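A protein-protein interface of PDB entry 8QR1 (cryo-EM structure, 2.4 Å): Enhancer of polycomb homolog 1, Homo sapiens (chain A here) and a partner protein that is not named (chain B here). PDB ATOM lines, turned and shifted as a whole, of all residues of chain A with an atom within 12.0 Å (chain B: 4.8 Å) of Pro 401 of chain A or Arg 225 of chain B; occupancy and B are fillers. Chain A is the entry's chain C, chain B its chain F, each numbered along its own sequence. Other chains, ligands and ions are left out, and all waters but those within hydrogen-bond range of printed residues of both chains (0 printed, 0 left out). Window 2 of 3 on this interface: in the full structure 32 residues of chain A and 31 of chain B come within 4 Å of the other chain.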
ATOM      1  N   ASP A 397      42.497 -23.852   7.175  1.00  0.00           N
ATOM      2  CA  ASP A 397      41.022 -23.903   6.965  1.00  0.00           C
ATOM      3  C   ASP A 397      40.705 -24.395   5.539  1.00  0.00           C
ATOM      4  O   ASP A 397      40.600 -23.579   4.621  1.00  0.00           O
ATOM      5  CB  ASP A 397      40.403 -22.526   7.222  1.00  0.00           C
ATOM      6  CG  ASP A 397      40.953 -21.868   8.472  1.00  0.00           C
ATOM      7  OD1 ASP A 397      40.146 -21.388   9.296  1.00  0.00           O
ATOM      8  OD2 ASP A 397      42.191 -21.827   8.629  1.00  0.00           O
ATOM      9  N   PRO A 398      40.584 -25.718   5.336  1.00  0.00           N
ATOM     10  CA  PRO A 398      40.301 -26.205   3.972  1.00  0.00           C
ATOM     11  C   PRO A 398      38.969 -25.737   3.417  1.00  0.00           C
ATOM     12  O   PRO A 398      38.901 -25.323   2.253  1.00  0.00           O
ATOM     13  CB  PRO A 398      40.336 -27.732   4.131  1.00  0.00           C
ATOM     14  CG  PRO A 398      41.118 -27.978   5.350  1.00  0.00           C
ATOM     15  CD  PRO A 398      40.797 -26.845   6.262  1.00  0.00           C
ATOM     16  N   ASP A 399      37.910 -25.776   4.226  1.00  0.00           N
ATOM     17  CA  ASP A 399      36.562 -25.436   3.791  1.00  0.00           C
ATOM     18  C   ASP A 399      36.200 -23.977   4.057  1.00  0.00           C
ATOM     19  O   ASP A 399      35.047 -23.590   3.848  1.00  0.00           O
ATOM     20  CB  ASP A 399      35.548 -26.356   4.468  1.00  0.00           C
ATOM     21  CG  ASP A 399      35.753 -27.815   4.116  1.00  0.00           C
ATOM     22  OD1 ASP A 399      36.322 -28.099   3.041  1.00  0.00           O
ATOM     23  OD2 ASP A 399      35.341 -28.681   4.915  1.00  0.00           O
ATOM     24  N   GLY A 400      37.148 -23.157   4.509  1.00  0.00           N
ATOM     25  CA  GLY A 400      36.876 -21.759   4.725  1.00  0.00           C
ATOM     26  C   GLY A 400      36.015 -21.542   5.956  1.00  0.00           C
ATOM     27  O   GLY A 400      36.112 -22.298   6.928  1.00  0.00           O
ATOM     28  N   PRO A 401      35.166 -20.506   5.960  1.00  0.00           N
ATOM     29  CA  PRO A 401      34.237 -20.342   7.092  1.00  0.00           C
ATOM     30  C   PRO A 401      33.253 -21.484   7.253  1.00  0.00           C
ATOM     31  O   PRO A 401      32.753 -21.690   8.364  1.00  0.00           O
ATOM     32  CB  PRO A 401      33.508 -19.034   6.764  1.00  0.00           C
ATOM     33  CG  PRO A 401      34.403 -18.313   5.853  1.00  0.00           C
ATOM     34  CD  PRO A 401      35.090 -19.354   5.044  1.00  0.00           C
ATOM     35  N   PHE A 402      32.975 -22.243   6.194  1.00  0.00           N
ATOM     36  CA  PHE A 402      31.917 -23.239   6.189  1.00  0.00           C
ATOM     37  C   PHE A 402      32.404 -24.620   6.610  1.00  0.00           C
ATOM     38  O   PHE A 402      31.844 -25.630   6.173  1.00  0.00           O
ATOM     39  CB  PHE A 402      31.280 -23.294   4.803  1.00  0.00           C
ATOM     40  CG  PHE A 402      30.875 -21.950   4.285  1.00  0.00           C
ATOM     41  CD1 PHE A 402      29.745 -21.323   4.768  1.00  0.00           C
ATOM     42  CD2 PHE A 402      31.637 -21.303   3.336  1.00  0.00           C
ATOM     43  CE1 PHE A 402      29.376 -20.085   4.303  1.00  0.00           C
ATOM     44  CE2 PHE A 402      31.271 -20.062   2.871  1.00  0.00           C
ATOM     45  CZ  PHE A 402      30.140 -19.454   3.354  1.00  0.00           C
ATOM     46  N   ALA A 403      33.437 -24.684   7.445  1.00  0.00           N
ATOM     47  CA  ALA A 403      33.841 -25.951   8.032  1.00  0.00           C
ATOM     48  C   ALA A 403      32.788 -26.427   9.022  1.00  0.00           C
ATOM     49  O   ALA A 403      32.152 -25.625   9.712  1.00  0.00           O
ATOM     50  CB  ALA A 403      35.191 -25.805   8.727  1.00  0.00           C
ATOM     51  N   PHE A 404      32.610 -27.745   9.089  1.00  0.00           N
ATOM     52  CA  PHE A 404      31.587 -28.361   9.933  1.00  0.00           C
ATOM     53  C   PHE A 404      32.142 -28.486  11.350  1.00  0.00           C
ATOM     54  O   PHE A 404      32.627 -29.535  11.779  1.00  0.00           O
ATOM     55  CB  PHE A 404      31.175 -29.711   9.352  1.00  0.00           C
ATOM     56  CG  PHE A 404      30.118 -30.460  10.146  1.00  0.00           C
ATOM     57  CD1 PHE A 404      29.162 -29.809  10.911  1.00  0.00           C
ATOM     58  CD2 PHE A 404      30.087 -31.840  10.102  1.00  0.00           C
ATOM     59  CE1 PHE A 404      28.222 -30.518  11.617  1.00  0.00           C
ATOM     60  CE2 PHE A 404      29.144 -32.548  10.808  1.00  0.00           C
ATOM     61  CZ  PHE A 404      28.211 -31.887  11.563  1.00  0.00           C
ATOM     62  N   ARG A 405      32.056 -27.380  12.088  1.00  0.00           N
ATOM     63  CA  ARG A 405      32.398 -27.365  13.504  1.00  0.00           C
ATOM     64  C   ARG A 405      31.233 -27.928  14.304  1.00  0.00           C
ATOM     65  O   ARG A 405      30.270 -27.216  14.602  1.00  0.00           O
ATOM     66  CB  ARG A 405      32.724 -25.940  13.977  1.00  0.00           C
ATOM     67  CG  ARG A 405      34.139 -25.360  13.699  1.00  0.00           C
ATOM     68  CD  ARG A 405      35.314 -26.350  13.744  1.00  0.00           C
ATOM     69  NE  ARG A 405      35.335 -27.141  14.973  1.00  0.00           N
ATOM     70  CZ  ARG A 405      35.621 -26.677  16.184  1.00  0.00           C
ATOM     71  NH1 ARG A 405      35.970 -25.415  16.389  1.00  0.00           N
ATOM     72  NH2 ARG A 405      35.557 -27.504  17.224  1.00  0.00           N
ATOM     73  N   ARG A 406      31.319 -29.207  14.650  1.00  0.00           N
ATOM     74  CA  ARG A 406      30.253 -29.868  15.386  1.00  0.00           C
ATOM     75  C   ARG A 406      30.160 -29.314  16.802  1.00  0.00           C
ATOM     76  O   ARG A 406      31.149 -28.844  17.367  1.00  0.00           O
ATOM     77  CB  ARG A 406      30.514 -31.376  15.407  1.00  0.00           C
ATOM     78  CG  ARG A 406      29.457 -32.234  16.084  1.00  0.00           C
ATOM     79  CD  ARG A 406      29.870 -33.687  16.065  1.00  0.00           C
ATOM     80  NE  ARG A 406      29.040 -34.516  16.932  1.00  0.00           N
ATOM     81  CZ  ARG A 406      29.330 -35.754  17.315  1.00  0.00           C
ATOM     82  NH1 ARG A 406      30.449 -36.361  16.944  1.00  0.00           N
ATOM     83  NH2 ARG A 406      28.472 -36.407  18.091  1.00  0.00           N
ATOM     84  N   LYS A 407      28.951 -29.357  17.358  1.00  0.00           N
ATOM     85  CA  LYS A 407      28.677 -28.984  18.738  1.00  0.00           C
ATOM     86  C   LYS A 407      28.136 -30.194  19.486  1.00  0.00           C
ATOM     87  O   LYS A 407      27.402 -31.009  18.920  1.00  0.00           O
ATOM     88  CB  LYS A 407      27.678 -27.828  18.814  1.00  0.00           C
ATOM     89  CG  LYS A 407      27.369 -27.383  20.231  1.00  0.00           C
ATOM     90  CD  LYS A 407      26.825 -25.961  20.293  1.00  0.00           C
ATOM     91  CE  LYS A 407      27.924 -24.914  20.191  1.00  0.00           C
ATOM     92  NZ  LYS A 407      27.426 -23.557  20.540  1.00  0.00           N
ATOM     93  N   ALA A 408      28.511 -30.306  20.757  1.00  0.00           N
ATOM     94  CA  ALA A 408      28.161 -31.479  21.543  1.00  0.00           C
ATOM     95  C   ALA A 408      26.661 -31.545  21.791  1.00  0.00           C
ATOM     96  O   ALA A 408      26.013 -30.534  22.075  1.00  0.00           O
ATOM     97  CB  ALA A 408      28.913 -31.459  22.871  1.00  0.00           C
ATOM     98  N   CYS A 410      24.264 -32.180  19.674  1.00  0.00           N
ATOM     99  CA  CYS A 410      23.428 -31.923  18.515  1.00  0.00           C
ATOM    100  C   CYS A 410      23.404 -33.132  17.585  1.00  0.00           C
ATOM    101  O   CYS A 410      24.290 -33.992  17.613  1.00  0.00           O
ATOM    102  CB  CYS A 410      23.935 -30.699  17.760  1.00  0.00           C
ATOM    103  SG  CYS A 410      23.982 -29.189  18.737  1.00  0.00           S
ATOM    104  N   TYR A 412      22.426 -34.094  13.298  1.00  0.00           N
ATOM    105  CA  TYR A 412      22.499 -33.460  11.991  1.00  0.00           C
ATOM    106  C   TYR A 412      21.963 -34.396  10.919  1.00  0.00           C
ATOM    107  O   TYR A 412      22.111 -35.617  11.013  1.00  0.00           O
ATOM    108  CB  TYR A 412      23.938 -33.065  11.657  1.00  0.00           C
ATOM    109  CG  TYR A 412      24.574 -32.127  12.654  1.00  0.00           C
ATOM    110  CD1 TYR A 412      25.241 -32.614  13.767  1.00  0.00           C
ATOM    111  CD2 TYR A 412      24.514 -30.757  12.480  1.00  0.00           C
ATOM    112  CE1 TYR A 412      25.825 -31.762  14.677  1.00  0.00           C
ATOM    113  CE2 TYR A 412      25.094 -29.899  13.386  1.00  0.00           C
ATOM    114  CZ  TYR A 412      25.749 -30.406  14.480  1.00  0.00           C
ATOM    115  OH  TYR A 412      26.327 -29.547  15.381  1.00  0.00           O
ATOM    116  N   PRO A 415      23.291 -33.979   3.674  1.00  0.00           N
ATOM    117  CA  PRO A 415      22.684 -33.461   2.443  1.00  0.00           C
ATOM    118  C   PRO A 415      22.670 -34.495   1.332  1.00  0.00           C
ATOM    119  O   PRO A 415      23.407 -35.483   1.357  1.00  0.00           O
ATOM    120  CB  PRO A 415      23.586 -32.282   2.083  1.00  0.00           C
ATOM    121  CG  PRO A 415      24.893 -32.674   2.581  1.00  0.00           C
ATOM    122  CD  PRO A 415      24.677 -33.496   3.812  1.00  0.00           C
ATOM    123  N   GLY B 221      24.729 -20.352  14.636  1.00  0.00           N
ATOM    124  CA  GLY B 221      25.792 -20.016  13.707  1.00  0.00           C
ATOM    125  C   GLY B 221      25.963 -21.053  12.617  1.00  0.00           C
ATOM    126  O   GLY B 221      26.228 -20.713  11.460  1.00  0.00           O
ATOM    127  N   HIS B 222      25.807 -22.329  12.969  1.00  0.00           N
ATOM    128  CA  HIS B 222      25.895 -23.397  11.982  1.00  0.00           C
ATOM    129  C   HIS B 222      24.802 -23.254  10.932  1.00  0.00           C
ATOM    130  O   HIS B 222      25.057 -23.381   9.729  1.00  0.00           O
ATOM    131  CB  HIS B 222      25.796 -24.749  12.682  1.00  0.00           C
ATOM    132  CG  HIS B 222      25.768 -25.916  11.749  1.00  0.00           C
ATOM    133  ND1 HIS B 222      26.914 -26.515  11.276  1.00  0.00           N
ATOM    134  CD2 HIS B 222      24.734 -26.602  11.209  1.00  0.00           C
ATOM    135  CE1 HIS B 222      26.587 -27.516  10.479  1.00  0.00           C
ATOM    136  NE2 HIS B 222      25.270 -27.589  10.422  1.00  0.00           N
ATOM    137  N   GLU B 223      23.579 -22.966  11.375  1.00  0.00           N
ATOM    138  CA  GLU B 223      22.478 -22.773  10.443  1.00  0.00           C
ATOM    139  C   GLU B 223      22.706 -21.551   9.569  1.00  0.00           C
ATOM    140  O   GLU B 223      22.408 -21.573   8.370  1.00  0.00           O
ATOM    141  CB  GLU B 223      21.164 -22.641  11.207  1.00  0.00           C
ATOM    142  CG  GLU B 223      20.727 -23.901  11.923  1.00  0.00           C
ATOM    143  CD  GLU B 223      20.220 -24.966  10.978  1.00  0.00           C
ATOM    144  OE1 GLU B 223      21.052 -25.687  10.392  1.00  0.00           O
ATOM    145  OE2 GLU B 223      18.987 -25.083  10.816  1.00  0.00           O
ATOM    146  N   ARG B 224      23.233 -20.476  10.155  1.00  0.00           N
ATOM    147  CA  ARG B 224      23.484 -19.258   9.393  1.00  0.00           C
ATOM    148  C   ARG B 224      24.510 -19.509   8.299  1.00  0.00           C
ATOM    149  O   ARG B 224      24.327 -19.098   7.148  1.00  0.00           O
ATOM    150  CB  ARG B 224      23.979 -18.154  10.321  1.00  0.00           C
ATOM    151  CG  ARG B 224      22.889 -17.378  11.022  1.00  0.00           C
ATOM    152  CD  ARG B 224      23.382 -16.058  11.571  1.00  0.00           C
ATOM    153  NE  ARG B 224      24.261 -16.228  12.724  1.00  0.00           N
ATOM    154  CZ  ARG B 224      23.869 -16.358  13.984  1.00  0.00           C
ATOM    155  NH1 ARG B 224      22.594 -16.478  14.311  1.00  0.00           N
ATOM    156  NH2 ARG B 224      24.787 -16.391  14.945  1.00  0.00           N
ATOM    157  N   ARG B 225      25.594 -20.201   8.647  1.00  0.00           N
ATOM    158  CA  ARG B 225      26.620 -20.524   7.664  1.00  0.00           C
ATOM    159  C   ARG B 225      26.084 -21.462   6.592  1.00  0.00           C
ATOM    160  O   ARG B 225      26.432 -21.330   5.414  1.00  0.00           O
ATOM    161  CB  ARG B 225      27.825 -21.138   8.369  1.00  0.00           C
ATOM    162  CG  ARG B 225      28.605 -20.148   9.200  1.00  0.00           C
ATOM    163  CD  ARG B 225      29.909 -20.729   9.694  1.00  0.00           C
ATOM    164  NE  ARG B 225      29.721 -21.841  10.621  1.00  0.00           N
ATOM    165  CZ  ARG B 225      29.593 -21.740  11.940  1.00  0.00           C
ATOM    166  NH1 ARG B 225      29.573 -20.568  12.559  1.00  0.00           N
ATOM    167  NH2 ARG B 225      29.476 -22.848  12.663  1.00  0.00           N
ATOM    168  N   ARG B 226      25.237 -22.417   6.983  1.00  0.00           N
ATOM    169  CA  ARG B 226      24.631 -23.329   6.019  1.00  0.00           C
ATOM    170  C   ARG B 226      23.778 -22.575   5.007  1.00  0.00           C
ATOM    171  O   ARG B 226      23.895 -22.786   3.792  1.00  0.00           O
ATOM    172  CB  ARG B 226      23.789 -24.361   6.764  1.00  0.00           C
ATOM    173  CG  ARG B 226      23.385 -25.566   5.954  1.00  0.00           C
ATOM    174  CD  ARG B 226      22.276 -26.333   6.624  1.00  0.00           C
ATOM    175  NE  ARG B 226      20.972 -26.008   6.050  1.00  0.00           N
ATOM    176  CZ  ARG B 226      20.002 -25.299   6.618  1.00  0.00           C
ATOM    177  NH1 ARG B 226      20.108 -24.800   7.838  1.00  0.00           N
ATOM    178  NH2 ARG B 226      18.883 -25.081   5.939  1.00  0.00           N
ATOM    179  N   LYS B 227      22.913 -21.688   5.492  1.00  0.00           N
ATOM    180  CA  LYS B 227      22.037 -20.951   4.590  1.00  0.00           C
ATOM    181  C   LYS B 227      22.829 -19.960   3.747  1.00  0.00           C
ATOM    182  O   LYS B 227      22.484 -19.712   2.587  1.00  0.00           O
ATOM    183  CB  LYS B 227      20.937 -20.260   5.392  1.00  0.00           C
ATOM    184  CG  LYS B 227      20.048 -21.248   6.139  1.00  0.00           C
ATOM    185  CD  LYS B 227      18.581 -20.897   6.148  1.00  0.00           C
ATOM    186  CE  LYS B 227      18.278 -19.737   7.047  1.00  0.00           C
ATOM    187  NZ  LYS B 227      16.837 -19.416   6.968  1.00  0.00           N
ATOM    188  N   GLU B 228      23.911 -19.408   4.298  1.00  0.00           N
ATOM    189  CA  GLU B 228      24.782 -18.539   3.515  1.00  0.00           C
ATOM    190  C   GLU B 228      25.462 -19.305   2.388  1.00  0.00           C
ATOM    191  O   GLU B 228      25.575 -18.801   1.264  1.00  0.00           O
ATOM    192  CB  GLU B 228      25.821 -17.899   4.429  1.00  0.00           C
ATOM    193  CG  GLU B 228      26.424 -16.624   3.895  1.00  0.00           C
ATOM    194  CD  GLU B 228      27.897 -16.484   4.229  1.00  0.00           C
ATOM    195  OE1 GLU B 228      28.644 -15.924   3.400  1.00  0.00           O
ATOM    196  OE2 GLU B 228      28.308 -16.922   5.325  1.00  0.00           O
ATOM    197  N   GLN B 229      25.930 -20.522   2.672  1.00  0.00           N
ATOM    198  CA  GLN B 229      26.533 -21.346   1.629  1.00  0.00           C
ATOM    199  C   GLN B 229      25.512 -21.703   0.562  1.00  0.00           C
ATOM    200  O   GLN B 229      25.830 -21.709  -0.633  1.00  0.00           O
ATOM    201  CB  GLN B 229      27.124 -22.616   2.233  1.00  0.00           C
ATOM    202  CG  GLN B 229      27.812 -23.516   1.216  1.00  0.00           C
ATOM    203  CD  GLN B 229      28.725 -24.555   1.834  1.00  0.00           C
ATOM    204  OE1 GLN B 229      29.800 -24.833   1.308  1.00  0.00           O
ATOM    205  NE2 GLN B 229      28.280 -25.177   2.919  1.00  0.00           N
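The backbone NH (N) of Lys 407 of chain A lies within hydrogen-bond range of the side-chain hydroxyl (OH) of Tyr 412 of chain A, 3.3 Å away.
Among the printed residues, pairs that only touch across the chains: Pro 401 of chain A with Arg 225 of chain B, Phe 402 of chain A with Arg 225 of chain B, Phe 404 of chain A with His 222 of chain B, Phe 402 of chain A with Glu 228 of chain B, Tyr 412 of chain A with His 222 of chain B and Phe 402 of chain A with Gln 229 of chain B.
Of chain B, only Arg 225 comes within 4 Å of Pro 401 of chain A.
Of chain A, only Pro 401 (3.3 Å) and Phe 402 (3.4 Å) come within 4 Å of Arg 225 of chain B.
No residue of chain A comes within 4 Å of Gly 221 of chain B.
Printed residues of chain A within 4 Å of His 222 of chain B: Phe 404 (3.5 Å) and Tyr 412 (3.8 Å).
No residue of chain A comes within 4 Å of Arg 224 of chain B.
Of chain A, only Phe 402 comes within 4 Å of Glu 228 of chain B.
Of chain A, only Phe 402 (3.8 Å) comes within 4 Å of Gln 229 of chain B.
Of the printed residues of chain B, Phe 402 of chain A touches Arg 225, Glu 228 and Gln 229.
Of the printed residues of chain B, Phe 404 of chain A touches His 222 (3.5 Å).
Of the printed residues of chain B, Tyr 412 of chain A touches His 222 (3.8 Å).
The nearest residue of chain A that does not touch Arg 225 of chain B is Ala 403 of chain A (4.6 Å).
The nearest printed residue of chain B that does not touch Phe 404 of chain A is Arg 225 of chain B (6.4 Å).
Of the 15 printed residues of chain A, 4 touch a printed residue of chain B.
Hydrophobic or aromatic side chains of chain A within 4 Å of the printed part of chain B: Phe 402, Phe 404 and Tyr 412.
Printed residues of chain B that touch a printed residue of chain A: His 222, Arg 225, Glu 228 and Gln 229.
Hydrophobic or aromatic side chains of chain B within 4 Å of the printed part of chain A: His 222.
Along chain B the printed residues that touch a printed residue of chain A span positions 222 to 229.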
